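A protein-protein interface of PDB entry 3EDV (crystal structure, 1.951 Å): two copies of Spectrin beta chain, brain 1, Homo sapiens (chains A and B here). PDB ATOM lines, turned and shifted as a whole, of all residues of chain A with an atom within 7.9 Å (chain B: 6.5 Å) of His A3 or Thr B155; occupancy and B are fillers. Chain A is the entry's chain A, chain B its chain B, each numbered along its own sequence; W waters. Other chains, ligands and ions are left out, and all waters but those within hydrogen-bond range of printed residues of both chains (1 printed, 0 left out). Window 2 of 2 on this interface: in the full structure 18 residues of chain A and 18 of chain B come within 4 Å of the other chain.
A ring nitrogen (ND1) of His A3 sits close to the side-chain hydroxyl (OG1) of Thr B155, at 3.4 Å. OG1 of Thr B156 lies within hydrogen-bond range of OE1 of Gln A10.
OG1 of Thr B155 is in hydrogen-bond range of O of Gln B151 (3.0 Å). O of Arg B152 is in hydrogen-bond range of OG1 of Thr B156 (3.1 Å). ND1 of His B159 sits at hydrogen-bond distance from OD1 of Asp B160, 3.1 Å away.
Among the printed residues, merely in contact across the chains: Gln A10 with His B159 (3.3 Å), His A6 with Arg B152 (3.3 Å), Arg A7 with Thr B155 (3.7 Å), His A6 with Thr B155 (3.7 Å), Gln A10 with Thr B155 (3.8 Å), Leu A69 with His B159 (3.8 Å) and His A6 with Thr B156 (3.9 Å).
Of chain B, only Thr B155 (3.4 Å) comes within 4 Å of His A3. Of the printed residues of chain B, Gln A10 touches Thr B155, Thr B156 and His B159. Met B153 touches none of the printed residues of chain A. His B154 touches none of the printed residues of chain A. Thr B155 touches just these residues of chain A: His A3, His A6, Arg A7 and Gln A10. Of the printed residues of chain A, Thr B156 touches His A6 and Gln A10. The nearest residue of chain B that does not touch His A3 is Arg B212 (5.3 Å). The nearest residue of chain A that does not touch Thr B155 is Leu A69 (7.0 Å).
Hydrophobic or aromatic side chains of chain A within 4 Å of the printed part of chain B: His A3, His A6 and Leu A69. Along chain A the printed residues that touch a printed residue of chain B span positions 3 to 69. Printed residues of chain B that touch a printed residue of chain A: Arg B152, Thr B155, Thr B156 and His B159. Among the printed residues, 9 pairs touch across the chains. Among the printed residues, no Asp or Glu carboxylate lies within 4 Å of a Lys or Arg side-chain nitrogen of the other chain.
No position is printed for both chains. Of the 9 pairs that touch across the chains among the printed residues, none has its exchanged pair printed and touching as well.
Water W1 lies within hydrogen-bond range of a ring nitrogen (ND1) of His A6 (2.9 Å), the side-chain hydroxyl (OG1) of Thr B155 (2.9 Å) and a ring nitrogen (ND1) of His A3 (3.2 Å).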
ATOM      1  N   SER A   2      19.142 -17.004  -8.887  1.00  0.00           N
ATOM      2  CA  SER A   2      17.730 -17.268  -8.641  1.00  0.00           C
ATOM      3  C   SER A   2      17.544 -18.202  -7.450  1.00  0.00           C
ATOM      4  O   SER A   2      16.425 -18.406  -6.978  1.00  0.00           O
ATOM      5  CB  SER A   2      17.071 -17.866  -9.886  1.00  0.00           C
ATOM      6  OG  SER A   2      17.380 -17.106 -11.041  1.00  0.00           O
ATOM      7  N   HIS A   3      18.646 -18.768  -6.969  1.00  0.00           N
ATOM      8  CA  HIS A   3      18.682 -19.372  -5.643  1.00  0.00           C
ATOM      9  C   HIS A   3      18.120 -18.423  -4.590  1.00  0.00           C
ATOM     10  O   HIS A   3      17.244 -18.794  -3.809  1.00  0.00           O
ATOM     11  CB  HIS A   3      20.111 -19.777  -5.277  1.00  0.00           C
ATOM     12  CG  HIS A   3      20.292 -20.109  -3.828  1.00  0.00           C
ATOM     13  ND1 HIS A   3      19.767 -21.247  -3.255  1.00  0.00           N
ATOM     14  CD2 HIS A   3      20.941 -19.453  -2.837  1.00  0.00           C
ATOM     15  CE1 HIS A   3      20.084 -21.277  -1.973  1.00  0.00           C
ATOM     16  NE2 HIS A   3      20.796 -20.200  -1.694  1.00  0.00           N
ATOM     17  N   MET A   4      18.630 -17.195  -4.574  1.00  0.00           N
ATOM     18  CA  MET A   4      18.287 -16.236  -3.530  1.00  0.00           C
ATOM     19  C   MET A   4      16.805 -15.881  -3.572  1.00  0.00           C
ATOM     20  O   MET A   4      16.197 -15.589  -2.541  1.00  0.00           O
ATOM     21  CB  MET A   4      19.136 -14.971  -3.665  1.00  0.00           C
ATOM     22  CG  MET A   4      20.479 -15.046  -2.959  1.00  0.00           C
ATOM     23  SD  MET A   4      20.323 -15.438  -1.206  1.00  0.00           S
ATOM     24  CE  MET A   4      21.928 -14.924  -0.599  1.00  0.00           C
ATOM     25  N   ARG A   5      16.229 -15.907  -4.769  1.00  0.00           N
ATOM     26  CA  ARG A   5      14.795 -15.701  -4.934  1.00  0.00           C
ATOM     27  C   ARG A   5      13.998 -16.845  -4.313  1.00  0.00           C
ATOM     28  O   ARG A   5      12.985 -16.621  -3.651  1.00  0.00           O
ATOM     29  CB  ARG A   5      14.441 -15.557  -6.415  1.00  0.00           C
ATOM     30  CG  ARG A   5      12.954 -15.667  -6.712  1.00  0.00           C
ATOM     31  CD  ARG A   5      12.639 -15.227  -8.132  1.00  0.00           C
ATOM     32  NE  ARG A   5      11.222 -14.925  -8.310  1.00  0.00           N
ATOM     33  CZ  ARG A   5      10.684 -14.510  -9.453  1.00  0.00           C
ATOM     34  NH1 ARG A   5      11.446 -14.346 -10.525  1.00  0.00           N
ATOM     35  NH2 ARG A   5       9.383 -14.259  -9.523  1.00  0.00           N
ATOM     36  N   HIS A   6      14.464 -18.071  -4.532  1.00  0.00           N
ATOM     37  CA  HIS A   6      13.803 -19.249  -3.987  1.00  0.00           C
ATOM     38  C   HIS A   6      13.715 -19.180  -2.466  1.00  0.00           C
ATOM     39  O   HIS A   6      12.665 -19.444  -1.883  1.00  0.00           O
ATOM     40  CB  HIS A   6      14.539 -20.522  -4.413  1.00  0.00           C
ATOM     41  CG  HIS A   6      13.833 -21.785  -4.030  1.00  0.00           C
ATOM     42  ND1 HIS A   6      14.458 -23.013  -4.016  1.00  0.00           N
ATOM     43  CD2 HIS A   6      12.554 -22.010  -3.647  1.00  0.00           C
ATOM     44  CE1 HIS A   6      13.596 -23.940  -3.641  1.00  0.00           C
ATOM     45  NE2 HIS A   6      12.433 -23.358  -3.412  1.00  0.00           N
ATOM     46  N   ARG A   7      14.826 -18.822  -1.830  1.00  0.00           N
ATOM     47  CA  ARG A   7      14.876 -18.716  -0.377  1.00  0.00           C
ATOM     48  C   ARG A   7      13.942 -17.622   0.129  1.00  0.00           C
ATOM     49  O   ARG A   7      13.371 -17.733   1.214  1.00  0.00           O
ATOM     50  CB  ARG A   7      16.308 -18.443   0.091  1.00  0.00           C
ATOM     51  CG  ARG A   7      17.191 -19.679   0.140  1.00  0.00           C
ATOM     52  CD  ARG A   7      18.614 -19.326   0.539  1.00  0.00           C
ATOM     53  NE  ARG A   7      18.698 -18.885   1.928  1.00  0.00           N
ATOM     54  CZ  ARG A   7      19.823 -18.499   2.523  1.00  0.00           C
ATOM     55  NH1 ARG A   7      20.965 -18.499   1.848  1.00  0.00           N
ATOM     56  NH2 ARG A   7      19.806 -18.113   3.791  1.00  0.00           N
ATOM     57  N   LEU A   8      13.792 -16.566  -0.664  1.00  0.00           N
ATOM     58  CA  LEU A   8      12.935 -15.446  -0.292  1.00  0.00           C
ATOM     59  C   LEU A   8      11.465 -15.847  -0.310  1.00  0.00           C
ATOM     60  O   LEU A   8      10.724 -15.570   0.634  1.00  0.00           O
ATOM     61  CB  LEU A   8      13.168 -14.260  -1.231  1.00  0.00           C
ATOM     62  CG  LEU A   8      12.323 -13.012  -0.968  1.00  0.00           C
ATOM     63  CD1 LEU A   8      12.786 -12.305   0.297  1.00  0.00           C
ATOM     64  CD2 LEU A   8      12.370 -12.069  -2.161  1.00  0.00           C
ATOM     65  N   PHE A   9      11.047 -16.501  -1.389  1.00  0.00           N
ATOM     66  CA  PHE A   9       9.671 -16.967  -1.517  1.00  0.00           C
ATOM     67  C   PHE A   9       9.366 -18.070  -0.509  1.00  0.00           C
ATOM     68  O   PHE A   9       8.262 -18.141   0.032  1.00  0.00           O
ATOM     69  CB  PHE A   9       9.406 -17.468  -2.939  1.00  0.00           C
ATOM     70  CG  PHE A   9       8.927 -16.398  -3.878  1.00  0.00           C
ATOM     71  CD1 PHE A   9       7.578 -16.254  -4.156  1.00  0.00           C
ATOM     72  CD2 PHE A   9       9.825 -15.535  -4.484  1.00  0.00           C
ATOM     73  CE1 PHE A   9       7.134 -15.271  -5.020  1.00  0.00           C
ATOM     74  CE2 PHE A   9       9.387 -14.550  -5.348  1.00  0.00           C
ATOM     75  CZ  PHE A   9       8.040 -14.418  -5.616  1.00  0.00           C
ATOM     76  N   GLN A  10      10.351 -18.926  -0.261  1.00  0.00           N
ATOM     77  CA  GLN A  10      10.230 -19.956   0.765  1.00  0.00           C
ATOM     78  C   GLN A  10       9.966 -19.342   2.135  1.00  0.00           C
ATOM     79  O   GLN A  10       9.057 -19.763   2.851  1.00  0.00           O
ATOM     80  CB  GLN A  10      11.493 -20.819   0.810  1.00  0.00           C
ATOM     81  CG  GLN A  10      11.398 -22.101  -0.002  1.00  0.00           C
ATOM     82  CD  GLN A  10      12.339 -23.178   0.500  1.00  0.00           C
ATOM     83  OE1 GLN A  10      12.239 -24.340   0.104  1.00  0.00           O
ATOM     84  NE2 GLN A  10      13.261 -22.797   1.377  1.00  0.00           N
ATOM     85  N   LEU A  69      15.724 -18.228  10.231  1.00  0.00           N
ATOM     86  CA  LEU A  69      15.737 -18.216   8.753  1.00  0.00           C
ATOM     87  C   LEU A  69      15.770 -16.807   8.179  1.00  0.00           C
ATOM     88  O   LEU A  69      16.528 -16.516   7.249  1.00  0.00           O
ATOM     89  CB  LEU A  69      14.527 -18.961   8.205  1.00  0.00           C
ATOM     90  CG  LEU A  69      14.543 -20.482   8.372  1.00  0.00           C
ATOM     91  CD1 LEU A  69      13.118 -20.973   8.550  1.00  0.00           C
ATOM     92  CD2 LEU A  69      15.234 -21.163   7.161  1.00  0.00           C
ATOM     93  N   LEU A  73      19.082 -14.923   6.147  1.00  0.00           N
ATOM     94  CA  LEU A  73      18.992 -14.142   4.910  1.00  0.00           C
ATOM     95  C   LEU A  73      19.520 -12.695   5.027  1.00  0.00           C
ATOM     96  O   LEU A  73      20.321 -12.260   4.187  1.00  0.00           O
ATOM     97  CB  LEU A  73      17.582 -14.187   4.324  1.00  0.00           C
ATOM     98  CG  LEU A  73      17.265 -15.506   3.613  1.00  0.00           C
ATOM     99  CD1 LEU A  73      15.789 -15.669   3.468  1.00  0.00           C
ATOM    100  CD2 LEU A  73      17.973 -15.588   2.241  1.00  0.00           C
ATOM    101  N   HIS A  78      21.189 -10.605   1.737  1.00  0.00           N
ATOM    102  CA  HIS A  78      20.116 -10.768   0.756  1.00  0.00           C
ATOM    103  C   HIS A  78      19.682  -9.401   0.219  1.00  0.00           C
ATOM    104  O   HIS A  78      19.625  -8.424   0.974  1.00  0.00           O
ATOM    105  CB  HIS A  78      18.905 -11.498   1.348  1.00  0.00           C
ATOM    106  CG  HIS A  78      17.870 -11.841   0.315  1.00  0.00           C
ATOM    107  ND1 HIS A  78      17.051 -10.892  -0.258  1.00  0.00           N
ATOM    108  CD2 HIS A  78      17.561 -13.014  -0.286  1.00  0.00           C
ATOM    109  CE1 HIS A  78      16.277 -11.467  -1.162  1.00  0.00           C
ATOM    110  NE2 HIS A  78      16.563 -12.756  -1.196  1.00  0.00           N
ATOM    111  N   LEU B 150      17.676 -30.512  -8.234  1.00  0.00           N
ATOM    112  CA  LEU B 150      18.358 -30.952  -7.016  1.00  0.00           C
ATOM    113  C   LEU B 150      18.781 -29.789  -6.098  1.00  0.00           C
ATOM    114  O   LEU B 150      18.679 -29.902  -4.870  1.00  0.00           O
ATOM    115  CB  LEU B 150      19.556 -31.846  -7.346  1.00  0.00           C
ATOM    116  CG  LEU B 150      19.168 -33.231  -7.897  1.00  0.00           C
ATOM    117  CD1 LEU B 150      20.402 -33.876  -8.487  1.00  0.00           C
ATOM    118  CD2 LEU B 150      18.534 -34.154  -6.855  1.00  0.00           C
ATOM    119  N   GLN B 151      19.231 -28.680  -6.695  1.00  0.00           N
ATOM    120  CA  GLN B 151      19.598 -27.481  -5.925  1.00  0.00           C
ATOM    121  C   GLN B 151      18.389 -26.966  -5.168  1.00  0.00           C
ATOM    122  O   GLN B 151      18.488 -26.632  -4.003  1.00  0.00           O
ATOM    123  CB  GLN B 151      20.165 -26.352  -6.807  1.00  0.00           C
ATOM    124  CG  GLN B 151      21.587 -26.577  -7.343  1.00  0.00           C
ATOM    125  CD  GLN B 151      22.008 -25.516  -8.355  1.00  0.00           C
ATOM    126  OE1 GLN B 151      21.164 -24.808  -8.921  1.00  0.00           O
ATOM    127  NE2 GLN B 151      23.323 -25.394  -8.584  1.00  0.00           N
ATOM    128  N   ARG B 152      17.240 -26.925  -5.835  1.00  0.00           N
ATOM    129  CA  ARG B 152      15.992 -26.467  -5.214  1.00  0.00           C
ATOM    130  C   ARG B 152      15.466 -27.426  -4.129  1.00  0.00           C
ATOM    131  O   ARG B 152      14.880 -26.985  -3.139  1.00  0.00           O
ATOM    132  CB  ARG B 152      14.897 -26.263  -6.269  1.00  0.00           C
ATOM    133  CG  ARG B 152      15.126 -25.006  -7.103  1.00  0.00           C
ATOM    134  CD  ARG B 152      14.387 -25.079  -8.416  1.00  0.00           C
ATOM    135  NE  ARG B 152      12.954 -25.100  -8.193  1.00  0.00           N
ATOM    136  CZ  ARG B 152      12.263 -24.095  -7.673  1.00  0.00           C
ATOM    137  NH1 ARG B 152      12.886 -22.974  -7.328  1.00  0.00           N
ATOM    138  NH2 ARG B 152      10.944 -24.207  -7.507  1.00  0.00           N
ATOM    139  N   MET B 153      15.673 -28.728  -4.331  1.00  0.00           N
ATOM    140  CA  MET B 153      15.313 -29.725  -3.333  1.00  0.00           C
ATOM    141  C   MET B 153      16.206 -29.545  -2.110  1.00  0.00           C
ATOM    142  O   MET B 153      15.764 -29.719  -0.984  1.00  0.00           O
ATOM    143  CB  MET B 153      15.460 -31.144  -3.883  1.00  0.00           C
ATOM    144  CG  MET B 153      14.392 -31.541  -4.897  1.00  0.00           C
ATOM    145  SD  MET B 153      14.558 -33.217  -5.577  1.00  0.00           S
ATOM    146  CE  MET B 153      14.287 -34.171  -4.084  1.00  0.00           C
ATOM    147  N   HIS B 154      17.458 -29.179  -2.336  1.00  0.00           N
ATOM    148  CA  HIS B 154      18.394 -29.056  -1.246  1.00  0.00           C
ATOM    149  C   HIS B 154      18.091 -27.816  -0.442  1.00  0.00           C
ATOM    150  O   HIS B 154      18.152 -27.835   0.786  1.00  0.00           O
ATOM    151  CB  HIS B 154      19.840 -29.010  -1.715  1.00  0.00           C
ATOM    152  CG  HIS B 154      20.808 -29.110  -0.582  1.00  0.00           C
ATOM    153  ND1 HIS B 154      20.810 -30.182   0.281  1.00  0.00           N
ATOM    154  CD2 HIS B 154      21.737 -28.250  -0.116  1.00  0.00           C
ATOM    155  CE1 HIS B 154      21.734 -29.999   1.209  1.00  0.00           C
ATOM    156  NE2 HIS B 154      22.316 -28.835   0.990  1.00  0.00           N
ATOM    157  N   THR B 155      17.740 -26.749  -1.153  1.00  0.00           N
ATOM    158  CA  THR B 155      17.310 -25.519  -0.520  1.00  0.00           C
ATOM    159  C   THR B 155      16.123 -25.786   0.408  1.00  0.00           C
ATOM    160  O   THR B 155      16.099 -25.333   1.551  1.00  0.00           O
ATOM    161  CB  THR B 155      17.099 -24.404  -1.583  1.00  0.00           C
ATOM    162  OG1 THR B 155      18.364 -24.150  -2.244  1.00  0.00           O
ATOM    163  CG2 THR B 155      16.608 -23.138  -0.948  1.00  0.00           C
ATOM    164  N   THR B 156      15.178 -26.595  -0.046  1.00  0.00           N
ATOM    165  CA  THR B 156      14.063 -27.007   0.820  1.00  0.00           C
ATOM    166  C   THR B 156      14.495 -27.891   2.017  1.00  0.00           C
ATOM    167  O   THR B 156      14.003 -27.720   3.128  1.00  0.00           O
ATOM    168  CB  THR B 156      12.920 -27.644  -0.031  1.00  0.00           C
ATOM    169  OG1 THR B 156      12.579 -26.729  -1.085  1.00  0.00           O
ATOM    170  CG2 THR B 156      11.675 -27.920   0.805  1.00  0.00           C
ATOM    171  N   PHE B 157      15.407 -28.827   1.789  1.00  0.00           N
ATOM    172  CA  PHE B 157      15.955 -29.667   2.854  1.00  0.00           C
ATOM    173  C   PHE B 157      16.590 -28.797   3.963  1.00  0.00           C
ATOM    174  O   PHE B 157      16.305 -28.957   5.166  1.00  0.00           O
ATOM    175  CB  PHE B 157      16.963 -30.646   2.214  1.00  0.00           C
ATOM    176  CG  PHE B 157      17.515 -31.690   3.156  1.00  0.00           C
ATOM    177  CD1 PHE B 157      17.042 -32.986   3.124  1.00  0.00           C
ATOM    178  CD2 PHE B 157      18.539 -31.384   4.040  1.00  0.00           C
ATOM    179  CE1 PHE B 157      17.574 -33.959   3.986  1.00  0.00           C
ATOM    180  CE2 PHE B 157      19.063 -32.336   4.891  1.00  0.00           C
ATOM    181  CZ  PHE B 157      18.601 -33.617   4.866  1.00  0.00           C
ATOM    182  N   GLU B 158      17.453 -27.875   3.548  1.00  0.00           N
ATOM    183  CA  GLU B 158      18.130 -26.983   4.481  1.00  0.00           C
ATOM    184  C   GLU B 158      17.131 -26.087   5.208  1.00  0.00           C
ATOM    185  O   GLU B 158      17.288 -25.803   6.395  1.00  0.00           O
ATOM    186  CB  GLU B 158      19.167 -26.129   3.750  1.00  0.00           C
ATOM    187  CG  GLU B 158      20.360 -26.914   3.228  1.00  0.00           C
ATOM    188  CD  GLU B 158      21.418 -26.023   2.608  1.00  0.00           C
ATOM    189  OE1 GLU B 158      21.057 -25.152   1.788  1.00  0.00           O
ATOM    190  OE2 GLU B 158      22.609 -26.193   2.940  1.00  0.00           O
ATOM    191  N   HIS B 159      16.107 -25.643   4.487  1.00  0.00           N
ATOM    192  CA  HIS B 159      14.939 -25.032   5.109  1.00  0.00           C
ATOM    193  C   HIS B 159      14.324 -25.956   6.155  1.00  0.00           C
ATOM    194  O   HIS B 159      13.959 -25.517   7.245  1.00  0.00           O
ATOM    195  CB  HIS B 159      13.896 -24.668   4.050  1.00  0.00           C
ATOM    196  CG  HIS B 159      12.714 -23.930   4.594  1.00  0.00           C
ATOM    197  ND1 HIS B 159      11.526 -24.555   4.910  1.00  0.00           N
ATOM    198  CD2 HIS B 159      12.536 -22.619   4.881  1.00  0.00           C
ATOM    199  CE1 HIS B 159      10.668 -23.660   5.367  1.00  0.00           C
ATOM    200  NE2 HIS B 159      11.255 -22.478   5.359  1.00  0.00           N
ATOM    201  N   ASP B 160      14.215 -27.235   5.815  1.00  0.00           N
ATOM    202  CA  ASP B 160      13.344 -28.149   6.546  1.00  0.00           C
ATOM    203  C   ASP B 160      14.070 -28.769   7.736  1.00  0.00           C
ATOM    204  O   ASP B 160      13.501 -29.576   8.471  1.00  0.00           O
ATOM    205  CB  ASP B 160      12.822 -29.248   5.619  1.00  0.00           C
ATOM    206  CG  ASP B 160      11.559 -28.840   4.885  1.00  0.00           C
ATOM    207  OD1 ASP B 160      11.204 -27.644   4.931  1.00  0.00           O
ATOM    208  OD2 ASP B 160      10.921 -29.716   4.264  1.00  0.00           O
ATOM    209  N   ARG B 212      25.539 -28.466  -0.720  1.00  0.00           N
ATOM    210  CA  ARG B 212      25.232 -27.175  -1.378  1.00  0.00           C
ATOM    211  C   ARG B 212      26.408 -26.792  -2.295  1.00  0.00           C
ATOM    212  O   ARG B 212      26.239 -26.572  -3.489  1.00  0.00           O
ATOM    213  CB  ARG B 212      24.952 -26.081  -0.326  1.00  0.00           C
ATOM    214  CG  ARG B 212      24.353 -24.797  -0.885  1.00  0.00           C
ATOM    215  CD  ARG B 212      24.484 -23.606   0.107  1.00  0.00           C
ATOM    216  NE  ARG B 212      25.876 -23.264   0.440  1.00  0.00           N
ATOM    217  CZ  ARG B 212      26.739 -22.608  -0.351  1.00  0.00           C
ATOM    218  NH1 ARG B 212      26.403 -22.183  -1.574  1.00  0.00           N
ATOM    219  NH2 ARG B 212      27.964 -22.386   0.089  1.00  0.00           N
HETATM  220  O   HOH W   1      17.305 -22.818  -4.651  1.00  0.00           O
